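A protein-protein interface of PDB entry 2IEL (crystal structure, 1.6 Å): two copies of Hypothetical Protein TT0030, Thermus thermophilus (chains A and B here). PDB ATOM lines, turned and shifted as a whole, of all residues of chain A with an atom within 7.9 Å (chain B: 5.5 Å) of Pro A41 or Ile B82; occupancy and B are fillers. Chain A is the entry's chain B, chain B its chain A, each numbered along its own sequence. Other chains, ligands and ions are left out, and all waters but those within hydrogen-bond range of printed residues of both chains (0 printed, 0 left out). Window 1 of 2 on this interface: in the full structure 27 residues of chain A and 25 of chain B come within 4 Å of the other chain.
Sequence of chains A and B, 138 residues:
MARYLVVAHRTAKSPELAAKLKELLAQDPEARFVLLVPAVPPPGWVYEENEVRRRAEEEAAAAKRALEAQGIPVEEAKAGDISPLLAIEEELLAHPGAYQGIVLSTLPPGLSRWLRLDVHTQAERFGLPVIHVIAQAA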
ATOM      1  N   PRO A  38     -18.923  21.776 -23.320  1.00  0.00           N
ATOM      2  CA  PRO A  38     -17.472  21.734 -23.440  1.00  0.00           C
ATOM      3  C   PRO A  38     -16.949  23.140 -23.681  1.00  0.00           C
ATOM      4  O   PRO A  38     -17.115  23.698 -24.777  1.00  0.00           O
ATOM      5  CB  PRO A  38     -17.256  20.833 -24.668  1.00  0.00           C
ATOM      6  CG  PRO A  38     -18.562  20.080 -24.837  1.00  0.00           C
ATOM      7  CD  PRO A  38     -19.583  21.113 -24.451  1.00  0.00           C
ATOM      8  N   ALA A  39     -16.327  23.704 -22.657  1.00  0.00           N
ATOM      9  CA  ALA A  39     -15.908  25.103 -22.706  1.00  0.00           C
ATOM     10  C   ALA A  39     -14.678  25.447 -21.869  1.00  0.00           C
ATOM     11  O   ALA A  39     -14.176  26.573 -21.960  1.00  0.00           O
ATOM     12  CB  ALA A  39     -17.092  26.013 -22.321  1.00  0.00           C
ATOM     13  N   VAL A  40     -14.194  24.512 -21.059  1.00  0.00           N
ATOM     14  CA  VAL A  40     -13.056  24.784 -20.184  1.00  0.00           C
ATOM     15  C   VAL A  40     -11.738  24.496 -20.908  1.00  0.00           C
ATOM     16  O   VAL A  40     -11.403  23.324 -21.162  1.00  0.00           O
ATOM     17  CB  VAL A  40     -13.123  23.963 -18.863  1.00  0.00           C
ATOM     18  CG1 VAL A  40     -11.978  24.360 -17.917  1.00  0.00           C
ATOM     19  CG2 VAL A  40     -14.470  24.165 -18.170  1.00  0.00           C
ATOM     20  N   PRO A  41     -10.975  25.557 -21.220  1.00  0.00           N
ATOM     21  CA  PRO A  41      -9.670  25.321 -21.835  1.00  0.00           C
ATOM     22  C   PRO A  41      -8.633  24.912 -20.782  1.00  0.00           C
ATOM     23  O   PRO A  41      -8.813  25.214 -19.597  1.00  0.00           O
ATOM     24  CB  PRO A  41      -9.319  26.678 -22.440  1.00  0.00           C
ATOM     25  CG  PRO A  41     -10.028  27.680 -21.575  1.00  0.00           C
ATOM     26  CD  PRO A  41     -11.233  26.995 -20.984  1.00  0.00           C
ATOM     27  N   PRO A  42      -7.550  24.240 -21.208  1.00  0.00           N
ATOM     28  CA  PRO A  42      -6.498  23.865 -20.275  1.00  0.00           C
ATOM     29  C   PRO A  42      -5.758  25.094 -19.749  1.00  0.00           C
ATOM     30  O   PRO A  42      -5.811  26.158 -20.384  1.00  0.00           O
ATOM     31  CB  PRO A  42      -5.557  22.997 -21.130  1.00  0.00           C
ATOM     32  CG  PRO A  42      -5.811  23.432 -22.519  1.00  0.00           C
ATOM     33  CD  PRO A  42      -7.252  23.791 -22.583  1.00  0.00           C
ATOM     34  N   PRO A  43      -5.079  24.953 -18.592  1.00  0.00           N
ATOM     35  CA  PRO A  43      -4.336  26.047 -17.970  1.00  0.00           C
ATOM     36  C   PRO A  43      -3.317  26.664 -18.920  1.00  0.00           C
ATOM     37  O   PRO A  43      -2.740  25.953 -19.740  1.00  0.00           O
ATOM     38  CB  PRO A  43      -3.605  25.359 -16.815  1.00  0.00           C
ATOM     39  CG  PRO A  43      -4.416  24.168 -16.501  1.00  0.00           C
ATOM     40  CD  PRO A  43      -4.992  23.710 -17.804  1.00  0.00           C
ATOM     41  N   GLY A  44      -3.109  27.974 -18.809  1.00  0.00           N
ATOM     42  CA  GLY A  44      -2.150  28.678 -19.655  1.00  0.00           C
ATOM     43  C   GLY A  44      -1.163  29.517 -18.863  1.00  0.00           C
ATOM     44  O   GLY A  44      -1.066  29.391 -17.630  1.00  0.00           O
ATOM     45  N   TYR A  47      -3.582  33.394 -18.032  1.00  0.00           N
ATOM     46  CA  TYR A  47      -4.877  33.315 -17.354  1.00  0.00           C
ATOM     47  C   TYR A  47      -5.124  32.009 -16.587  1.00  0.00           C
ATOM     48  O   TYR A  47      -4.219  31.205 -16.373  1.00  0.00           O
ATOM     49  CB  TYR A  47      -6.004  33.562 -18.360  1.00  0.00           C
ATOM     50  CG  TYR A  47      -5.960  34.937 -18.994  1.00  0.00           C
ATOM     51  CD1 TYR A  47      -5.377  35.137 -20.242  1.00  0.00           C
ATOM     52  CD2 TYR A  47      -6.494  36.040 -18.337  1.00  0.00           C
ATOM     53  CE1 TYR A  47      -5.332  36.404 -20.819  1.00  0.00           C
ATOM     54  CE2 TYR A  47      -6.457  37.306 -18.902  1.00  0.00           C
ATOM     55  CZ  TYR A  47      -5.876  37.482 -20.141  1.00  0.00           C
ATOM     56  OH  TYR A  47      -5.840  38.737 -20.696  1.00  0.00           O
ATOM     57  N   GLU A  49      -6.273  29.459 -14.141  1.00  0.00           N
ATOM     58  CA  GLU A  49      -7.130  28.279 -14.053  1.00  0.00           C
ATOM     59  C   GLU A  49      -8.479  28.621 -13.432  1.00  0.00           C
ATOM     60  O   GLU A  49      -9.521  28.225 -13.959  1.00  0.00           O
ATOM     61  CB  GLU A  49      -6.449  27.167 -13.256  1.00  0.00           C
ATOM     62  CG  GLU A  49      -7.184  25.827 -13.294  1.00  0.00           C
ATOM     63  CD  GLU A  49      -6.378  24.686 -12.703  1.00  0.00           C
ATOM     64  OE1 GLU A  49      -5.129  24.737 -12.754  1.00  0.00           O
ATOM     65  OE2 GLU A  49      -7.000  23.731 -12.193  1.00  0.00           O
ATOM     66  N   GLU A  51      -9.648  31.659 -13.291  1.00  0.00           N
ATOM     67  CA  GLU A  51     -10.217  32.640 -14.216  1.00  0.00           C
ATOM     68  C   GLU A  51     -10.913  32.002 -15.420  1.00  0.00           C
ATOM     69  O   GLU A  51     -12.054  32.347 -15.729  1.00  0.00           O
ATOM     70  CB  GLU A  51      -9.159  33.657 -14.681  1.00  0.00           C
ATOM     71  CG  GLU A  51      -9.549  34.415 -15.965  1.00  0.00           C
ATOM     72  CD  GLU A  51      -8.942  35.799 -16.082  1.00  0.00           C
ATOM     73  OE1 GLU A  51      -8.036  36.150 -15.288  1.00  0.00           O
ATOM     74  OE2 GLU A  51      -9.380  36.545 -16.984  1.00  0.00           O
ATOM     75  N   VAL A  52     -10.235  31.076 -16.096  1.00  0.00           N
ATOM     76  CA  VAL A  52     -10.803  30.480 -17.308  1.00  0.00           C
ATOM     77  C   VAL A  52     -11.980  29.557 -16.988  1.00  0.00           C
ATOM     78  O   VAL A  52     -12.921  29.462 -17.772  1.00  0.00           O
ATOM     79  CB  VAL A  52      -9.740  29.796 -18.233  1.00  0.00           C
ATOM     80  CG1 VAL A  52      -8.536  30.716 -18.433  1.00  0.00           C
ATOM     81  CG2 VAL A  52      -9.310  28.418 -17.712  1.00  0.00           C
ATOM     82  N   ARG A  53     -11.923  28.907 -15.826  1.00  0.00           N
ATOM     83  CA  ARG A  53     -13.021  28.068 -15.340  1.00  0.00           C
ATOM     84  C   ARG A  53     -14.272  28.913 -15.105  1.00  0.00           C
ATOM     85  O   ARG A  53     -15.366  28.559 -15.549  1.00  0.00           O
ATOM     86  CB  ARG A  53     -12.593  27.325 -14.062  1.00  0.00           C
ATOM     87  CG  ARG A  53     -13.724  26.836 -13.143  1.00  0.00           C
ATOM     88  CD  ARG A  53     -14.594  25.768 -13.783  1.00  0.00           C
ATOM     89  NE  ARG A  53     -13.898  24.494 -13.921  1.00  0.00           N
ATOM     90  CZ  ARG A  53     -14.470  23.364 -14.328  1.00  0.00           C
ATOM     91  NH1 ARG A  53     -13.740  22.260 -14.426  1.00  0.00           N
ATOM     92  NH2 ARG A  53     -15.763  23.336 -14.647  1.00  0.00           N
ATOM     93  N   ARG A  54     -14.080  30.037 -14.419  1.00  0.00           N
ATOM     94  CA  ARG A  54     -15.134  30.995 -14.135  1.00  0.00           C
ATOM     95  C   ARG A  54     -15.840  31.428 -15.419  1.00  0.00           C
ATOM     96  O   ARG A  54     -17.071  31.381 -15.511  1.00  0.00           O
ATOM     97  CB  ARG A  54     -14.510  32.209 -13.445  1.00  0.00           C
ATOM     98  CG  ARG A  54     -15.461  33.080 -12.713  1.00  0.00           C
ATOM     99  CD  ARG A  54     -14.704  34.114 -11.894  1.00  0.00           C
ATOM    100  NE  ARG A  54     -14.128  33.564 -10.661  1.00  0.00           N
ATOM    101  CZ  ARG A  54     -14.818  33.320  -9.541  1.00  0.00           C
ATOM    102  NH1 ARG A  54     -16.125  33.547  -9.481  1.00  0.00           N
ATOM    103  NH2 ARG A  54     -14.198  32.834  -8.477  1.00  0.00           N
ATOM    104  N   ARG A  55     -15.047  31.841 -16.409  1.00  0.00           N
ATOM    105  CA  ARG A  55     -15.565  32.228 -17.712  1.00  0.00           C
ATOM    106  C   ARG A  55     -16.318  31.069 -18.371  1.00  0.00           C
ATOM    107  O   ARG A  55     -17.359  31.277 -18.995  1.00  0.00           O
ATOM    108  CB  ARG A  55     -14.431  32.739 -18.612  1.00  0.00           C
ATOM    109  CG  ARG A  55     -13.853  34.105 -18.184  1.00  0.00           C
ATOM    110  CD  ARG A  55     -12.537  34.450 -18.887  1.00  0.00           C
ATOM    111  NE  ARG A  55     -12.670  34.607 -20.341  1.00  0.00           N
ATOM    112  CZ  ARG A  55     -12.798  35.773 -20.974  1.00  0.00           C
ATOM    113  NH1 ARG A  55     -12.821  36.913 -20.296  1.00  0.00           N
ATOM    114  NH2 ARG A  55     -12.905  35.800 -22.299  1.00  0.00           N
ATOM    115  N   ALA A  56     -15.797  29.848 -18.220  1.00  0.00           N
ATOM    116  CA  ALA A  56     -16.457  28.655 -18.768  1.00  0.00           C
ATOM    117  C   ALA A  56     -17.802  28.358 -18.107  1.00  0.00           C
ATOM    118  O   ALA A  56     -18.760  27.988 -18.788  1.00  0.00           O
ATOM    119  CB  ALA A  56     -15.545  27.432 -18.680  1.00  0.00           C
ATOM    120  N   GLY A  80     -17.540  21.655 -18.935  1.00  0.00           N
ATOM    121  CA  GLY A  80     -16.554  20.583 -18.985  1.00  0.00           C
ATOM    122  C   GLY A  80     -15.402  20.958 -19.894  1.00  0.00           C
ATOM    123  O   GLY A  80     -15.438  22.001 -20.561  1.00  0.00           O
ATOM    124  N   ASP A  81     -14.405  20.078 -19.952  1.00  0.00           N
ATOM    125  CA  ASP A  81     -13.237  20.243 -20.843  1.00  0.00           C
ATOM    126  C   ASP A  81     -13.678  20.659 -22.243  1.00  0.00           C
ATOM    127  O   ASP A  81     -14.716  20.221 -22.733  1.00  0.00           O
ATOM    128  CB  ASP A  81     -12.432  18.933 -20.885  1.00  0.00           C
ATOM    129  CG  ASP A  81     -11.071  19.095 -21.555  1.00  0.00           C
ATOM    130  OD1 ASP A  81     -11.044  19.186 -22.795  1.00  0.00           O
ATOM    131  OD2 ASP A  81     -10.045  19.145 -20.835  1.00  0.00           O
ATOM    132  N   ILE A  82     -12.889  21.520 -22.882  1.00  0.00           N
ATOM    133  CA  ILE A  82     -13.265  22.076 -24.195  1.00  0.00           C
ATOM    134  C   ILE A  82     -13.273  21.008 -25.313  1.00  0.00           C
ATOM    135  O   ILE A  82     -13.849  21.226 -26.385  1.00  0.00           O
ATOM    136  CB  ILE A  82     -12.372  23.295 -24.555  1.00  0.00           C
ATOM    137  CG1 ILE A  82     -12.977  24.108 -25.699  1.00  0.00           C
ATOM    138  CG2 ILE A  82     -10.922  22.858 -24.797  1.00  0.00           C
ATOM    139  CD1 ILE A  82     -12.679  25.565 -25.575  1.00  0.00           C
ATOM    140  N   SER A  83     -12.646  19.863 -25.043  1.00  0.00           N
ATOM    141  CA  SER A  83     -12.768  18.677 -25.908  1.00  0.00           C
ATOM    142  C   SER A  83     -14.012  17.925 -25.483  1.00  0.00           C
ATOM    143  O   SER A  83     -14.019  17.365 -24.373  1.00  0.00           O
ATOM    144  CB  SER A  83     -11.593  17.708 -25.713  1.00  0.00           C
ATOM    145  OG  SER A  83     -11.980  16.392 -26.148  1.00  0.00           O
ATOM    146  N   ARG A 113     -16.765  21.922 -35.806  1.00  0.00           N
ATOM    147  CA  ARG A 113     -15.451  21.476 -35.342  1.00  0.00           C
ATOM    148  C   ARG A 113     -15.591  20.066 -34.753  1.00  0.00           C
ATOM    149  O   ARG A 113     -14.738  19.203 -34.969  1.00  0.00           O
ATOM    150  CB  ARG A 113     -14.914  22.419 -34.268  1.00  0.00           C
ATOM    151  CG  ARG A 113     -14.454  23.777 -34.742  1.00  0.00           C
ATOM    152  CD  ARG A 113     -14.114  24.715 -33.572  1.00  0.00           C
ATOM    153  NE  ARG A 113     -12.981  24.279 -32.747  1.00  0.00           N
ATOM    154  CZ  ARG A 113     -13.080  23.608 -31.591  1.00  0.00           C
ATOM    155  NH1 ARG A 113     -14.267  23.289 -31.076  1.00  0.00           N
ATOM    156  NH2 ARG A 113     -11.987  23.282 -30.937  1.00  0.00           N
ATOM    157  N   LEU A 117     -13.636  16.519 -35.742  1.00  0.00           N
ATOM    158  CA  LEU A 117     -12.912  15.770 -34.711  1.00  0.00           C
ATOM    159  C   LEU A 117     -13.507  14.379 -34.479  1.00  0.00           C
ATOM    160  O   LEU A 117     -13.073  13.671 -33.575  1.00  0.00           O
ATOM    161  CB  LEU A 117     -12.904  16.564 -33.405  1.00  0.00           C
ATOM    162  CG  LEU A 117     -12.065  17.848 -33.415  1.00  0.00           C
ATOM    163  CD1 LEU A 117     -12.489  18.830 -32.304  1.00  0.00           C
ATOM    164  CD2 LEU A 117     -10.558  17.520 -33.361  1.00  0.00           C
ATOM    165  N   PRO B  38      -2.017  25.923 -29.632  1.00  0.00           N
ATOM    166  CA  PRO B  38      -3.450  25.667 -29.651  1.00  0.00           C
ATOM    167  C   PRO B  38      -4.080  26.341 -28.424  1.00  0.00           C
ATOM    168  O   PRO B  38      -3.884  25.909 -27.293  1.00  0.00           O
ATOM    169  CB  PRO B  38      -3.532  24.124 -29.625  1.00  0.00           C
ATOM    170  CG  PRO B  38      -2.167  23.659 -30.049  1.00  0.00           C
ATOM    171  CD  PRO B  38      -1.248  24.687 -29.422  1.00  0.00           C
ATOM    172  N   ALA B  39      -4.767  27.448 -28.666  1.00  0.00           N
ATOM    173  CA  ALA B  39      -5.286  28.280 -27.578  1.00  0.00           C
ATOM    174  C   ALA B  39      -6.601  28.994 -27.895  1.00  0.00           C
ATOM    175  O   ALA B  39      -7.201  29.584 -26.997  1.00  0.00           O
ATOM    176  CB  ALA B  39      -4.226  29.288 -27.124  1.00  0.00           C
ATOM    177  N   VAL B  40      -7.060  28.944 -29.143  1.00  0.00           N
ATOM    178  CA  VAL B  40      -8.281  29.669 -29.532  1.00  0.00           C
ATOM    179  C   VAL B  40      -9.552  28.821 -29.353  1.00  0.00           C
ATOM    180  O   VAL B  40      -9.806  27.879 -30.134  1.00  0.00           O
ATOM    181  CB  VAL B  40      -8.213  30.206 -30.984  1.00  0.00           C
ATOM    182  CG1 VAL B  40      -9.451  31.063 -31.307  1.00  0.00           C
ATOM    183  CG2 VAL B  40      -6.920  30.984 -31.212  1.00  0.00           C
ATOM    184  N   PRO B  41     -10.377  29.150 -28.333  1.00  0.00           N
ATOM    185  CA  PRO B  41     -11.650  28.445 -28.237  1.00  0.00           C
ATOM    186  C   PRO B  41     -12.671  28.944 -29.277  1.00  0.00           C
ATOM    187  O   PRO B  41     -12.550  30.072 -29.766  1.00  0.00           O
ATOM    188  CB  PRO B  41     -12.136  28.798 -26.830  1.00  0.00           C
ATOM    189  CG  PRO B  41     -11.541  30.098 -26.543  1.00  0.00           C
ATOM    190  CD  PRO B  41     -10.214  30.140 -27.250  1.00  0.00           C
ATOM    191  N   PRO B  42     -13.695  28.126 -29.588  1.00  0.00           N
ATOM    192  CA  PRO B  42     -14.692  28.590 -30.546  1.00  0.00           C
ATOM    193  C   PRO B  42     -15.560  29.723 -29.971  1.00  0.00           C
ATOM    194  O   PRO B  42     -15.511  29.977 -28.753  1.00  0.00           O
ATOM    195  CB  PRO B  42     -15.532  27.334 -30.832  1.00  0.00           C
ATOM    196  CG  PRO B  42     -15.316  26.438 -29.681  1.00  0.00           C
ATOM    197  CD  PRO B  42     -13.982  26.761 -29.094  1.00  0.00           C
ATOM    198  N   GLY B  80      -3.558  29.140 -32.535  1.00  0.00           N
ATOM    199  CA  GLY B  80      -4.494  28.431 -33.404  1.00  0.00           C
ATOM    200  C   GLY B  80      -5.629  27.814 -32.602  1.00  0.00           C
ATOM    201  O   GLY B  80      -5.702  28.002 -31.379  1.00  0.00           O
ATOM    202  N   ASP B  81      -6.515  27.093 -33.294  1.00  0.00           N
ATOM    203  CA  ASP B  81      -7.645  26.370 -32.666  1.00  0.00           C
ATOM    204  C   ASP B  81      -7.181  25.602 -31.442  1.00  0.00           C
ATOM    205  O   ASP B  81      -6.091  25.034 -31.436  1.00  0.00           O
ATOM    206  CB  ASP B  81      -8.289  25.401 -33.656  1.00  0.00           C
ATOM    207  CG  ASP B  81      -9.687  24.963 -33.215  1.00  0.00           C
ATOM    208  OD1 ASP B  81      -9.782  24.038 -32.382  1.00  0.00           O
ATOM    209  OD2 ASP B  81     -10.678  25.522 -33.720  1.00  0.00           O
ATOM    210  N   ILE B  82      -8.013  25.611 -30.396  1.00  0.00           N
ATOM    211  CA  ILE B  82      -7.683  24.942 -29.145  1.00  0.00           C
ATOM    212  C   ILE B  82      -7.502  23.408 -29.304  1.00  0.00           C
ATOM    213  O   ILE B  82      -6.838  22.770 -28.481  1.00  0.00           O
ATOM    214  CB  ILE B  82      -8.711  25.320 -28.048  1.00  0.00           C
ATOM    215  CG1 ILE B  82      -8.169  24.998 -26.652  1.00  0.00           C
ATOM    216  CG2 ILE B  82     -10.088  24.730 -28.357  1.00  0.00           C
ATOM    217  CD1 ILE B  82      -8.632  26.008 -25.622  1.00  0.00           C
ATOM    218  N   SER B  83      -8.048  22.842 -30.379  1.00  0.00           N
ATOM    219  CA  SER B  83      -7.733  21.469 -30.782  1.00  0.00           C
ATOM    220  C   SER B  83      -6.396  21.445 -31.517  1.00  0.00           C
ATOM    221  O   SER B  83      -6.302  22.029 -32.604  1.00  0.00           O
ATOM    222  CB  SER B  83      -8.805  20.902 -31.728  1.00  0.00           C
ATOM    223  OG  SER B  83      -8.257  19.777 -32.441  1.00  0.00           O
ATOM    224  N   PRO B  84      -5.382  20.743 -30.973  1.00  0.00           N
ATOM    225  CA  PRO B  84      -4.128  20.712 -31.730  1.00  0.00           C
ATOM    226  C   PRO B  84      -4.290  20.136 -33.137  1.00  0.00           C
ATOM    227  O   PRO B  84      -3.604  20.589 -34.061  1.00  0.00           O
ATOM    228  CB  PRO B  84      -3.209  19.826 -30.892  1.00  0.00           C
ATOM    229  CG  PRO B  84      -4.077  19.166 -29.901  1.00  0.00           C
ATOM    230  CD  PRO B  84      -5.293  19.968 -29.724  1.00  0.00           C
ATOM    231  N   ARG B 113      -3.663  15.849 -22.070  1.00  0.00           N
ATOM    232  CA  ARG B 113      -4.933  15.847 -22.776  1.00  0.00           C
ATOM    233  C   ARG B 113      -4.751  15.407 -24.241  1.00  0.00           C
ATOM    234  O   ARG B 113      -5.544  14.623 -24.769  1.00  0.00           O
ATOM    235  CB  ARG B 113      -5.566  17.231 -22.754  1.00  0.00           C
ATOM    236  CG  ARG B 113      -6.101  17.694 -21.394  1.00  0.00           C
ATOM    237  CD  ARG B 113      -6.565  19.147 -21.414  1.00  0.00           C
ATOM    238  NE  ARG B 113      -7.725  19.386 -22.270  1.00  0.00           N
ATOM    239  CZ  ARG B 113      -7.665  19.879 -23.508  1.00  0.00           C
ATOM    240  NH1 ARG B 113      -6.494  20.198 -24.042  1.00  0.00           N
ATOM    241  NH2 ARG B 113      -8.781  20.074 -24.199  1.00  0.00           N
ATOM    242  N   TRP B 114      -3.722  15.934 -24.909  1.00  0.00           N
ATOM    243  CA  TRP B 114      -3.504  15.589 -26.307  1.00  0.00           C
ATOM    244  C   TRP B 114      -3.228  14.098 -26.513  1.00  0.00           C
ATOM    245  O   TRP B 114      -3.707  13.526 -27.475  1.00  0.00           O
ATOM    246  CB  TRP B 114      -2.390  16.427 -26.930  1.00  0.00           C
ATOM    247  CG  TRP B 114      -2.625  17.914 -26.849  1.00  0.00           C
ATOM    248  CD1 TRP B 114      -3.776  18.564 -26.461  1.00  0.00           C
ATOM    249  CD2 TRP B 114      -1.680  18.943 -27.194  1.00  0.00           C
ATOM    250  NE1 TRP B 114      -3.595  19.931 -26.550  1.00  0.00           N
ATOM    251  CE2 TRP B 114      -2.324  20.185 -26.995  1.00  0.00           C
ATOM    252  CE3 TRP B 114      -0.355  18.930 -27.652  1.00  0.00           C
ATOM    253  CZ2 TRP B 114      -1.674  21.418 -27.210  1.00  0.00           C
ATOM    254  CZ3 TRP B 114       0.298  20.167 -27.869  1.00  0.00           C
ATOM    255  CH2 TRP B 114      -0.384  21.383 -27.677  1.00  0.00           C
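Pro A42 touches Arg B113, and with the chains exchanged Arg A113 touches Pro B42. Ile B82 touches its own counterpart, Ile A82. Ile A82 touches Arg B113, and with the chains exchanged Arg A113 touches Ile B82. Ser A83 touches Arg B113, but with the chains exchanged Arg A113 does not touch Ser B83 (4.003 Å). 10 positions are printed for both chains.
The side-chain carboxylate (OD1) of Asp B81 is in salt-bridge range of the guanidinium group (NH2) of Arg A113. NE of Arg B113 is in salt-bridge range of OD2 of Asp A81 (2.7 Å).
Printed residues of chain A within 4 Å of Ile B82: Pro A41, Ile A82 and Arg A113. Of the printed residues of chain B, Pro A42 touches Arg B113. Of the printed residues of chain B, Asp A81 touches Arg B113 (2.7 Å). Of the printed residues of chain A, Pro B41 touches Ile A82. Of the printed residues of chain A, Arg B113 touches Pro A42 (3.6 Å), Asp A81 (2.7 Å), Ile A82 (3.6 Å) and Ser A83 (3.96 Å). Of the printed residues of chain B, Leu A117 touches Ser B83. Val A40 touches none of the printed residues of chain B. Pro B84 touches none of the printed residues of chain A. The nearest printed residue of chain B that does not touch Pro A41 is Pro B41 (5.6 Å). The nearest printed residue of chain A that does not touch Ile B82 is Pro A42 (4.01 Å). The nearest printed residue of chain A that does not touch Asp B81 is Leu A117 (5.9 Å).
O of Val B40 is in hydrogen-bond range of N of Ile B82 (2.9 Å). The side-chain carboxylate (OD1) of Asp B81 lies within hydrogen-bond range of the backbone NH (N) of Ser B83 (2.9 Å). The side-chain carboxylate (OD1) of Asp A81 sits at hydrogen-bond distance from the backbone NH (N) of Ser A83 (2.8 Å). The backbone NH of Ile A82 sits at hydrogen-bond distance from the backbone carbonyl oxygen of Val A40 (2.9 Å).
Among the printed residues, merely in contact across the chains: Pro A41 with Ile B82 (3.3 Å), Pro A42 with Arg B113 (3.6 Å), Ile A82 with Pro B41 (3.5 Å), Ile A82 with Pro B42 (3.9 Å), Ile A82 with Ile B82 (3.9 Å), Ile A82 with Arg B113 (3.6 Å), Ser A83 with Arg B113 (3.96 Å), Arg A113 with Pro B42 (3.6 Å), Arg A113 with Ile B82 (3.5 Å) and Leu A117 with Ser B83 (3.4 Å).
Hydrophobic or aromatic side chains of chain A that line the printed part of chain B: Pro A41, Pro A42, Ile A82 and Leu A117.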
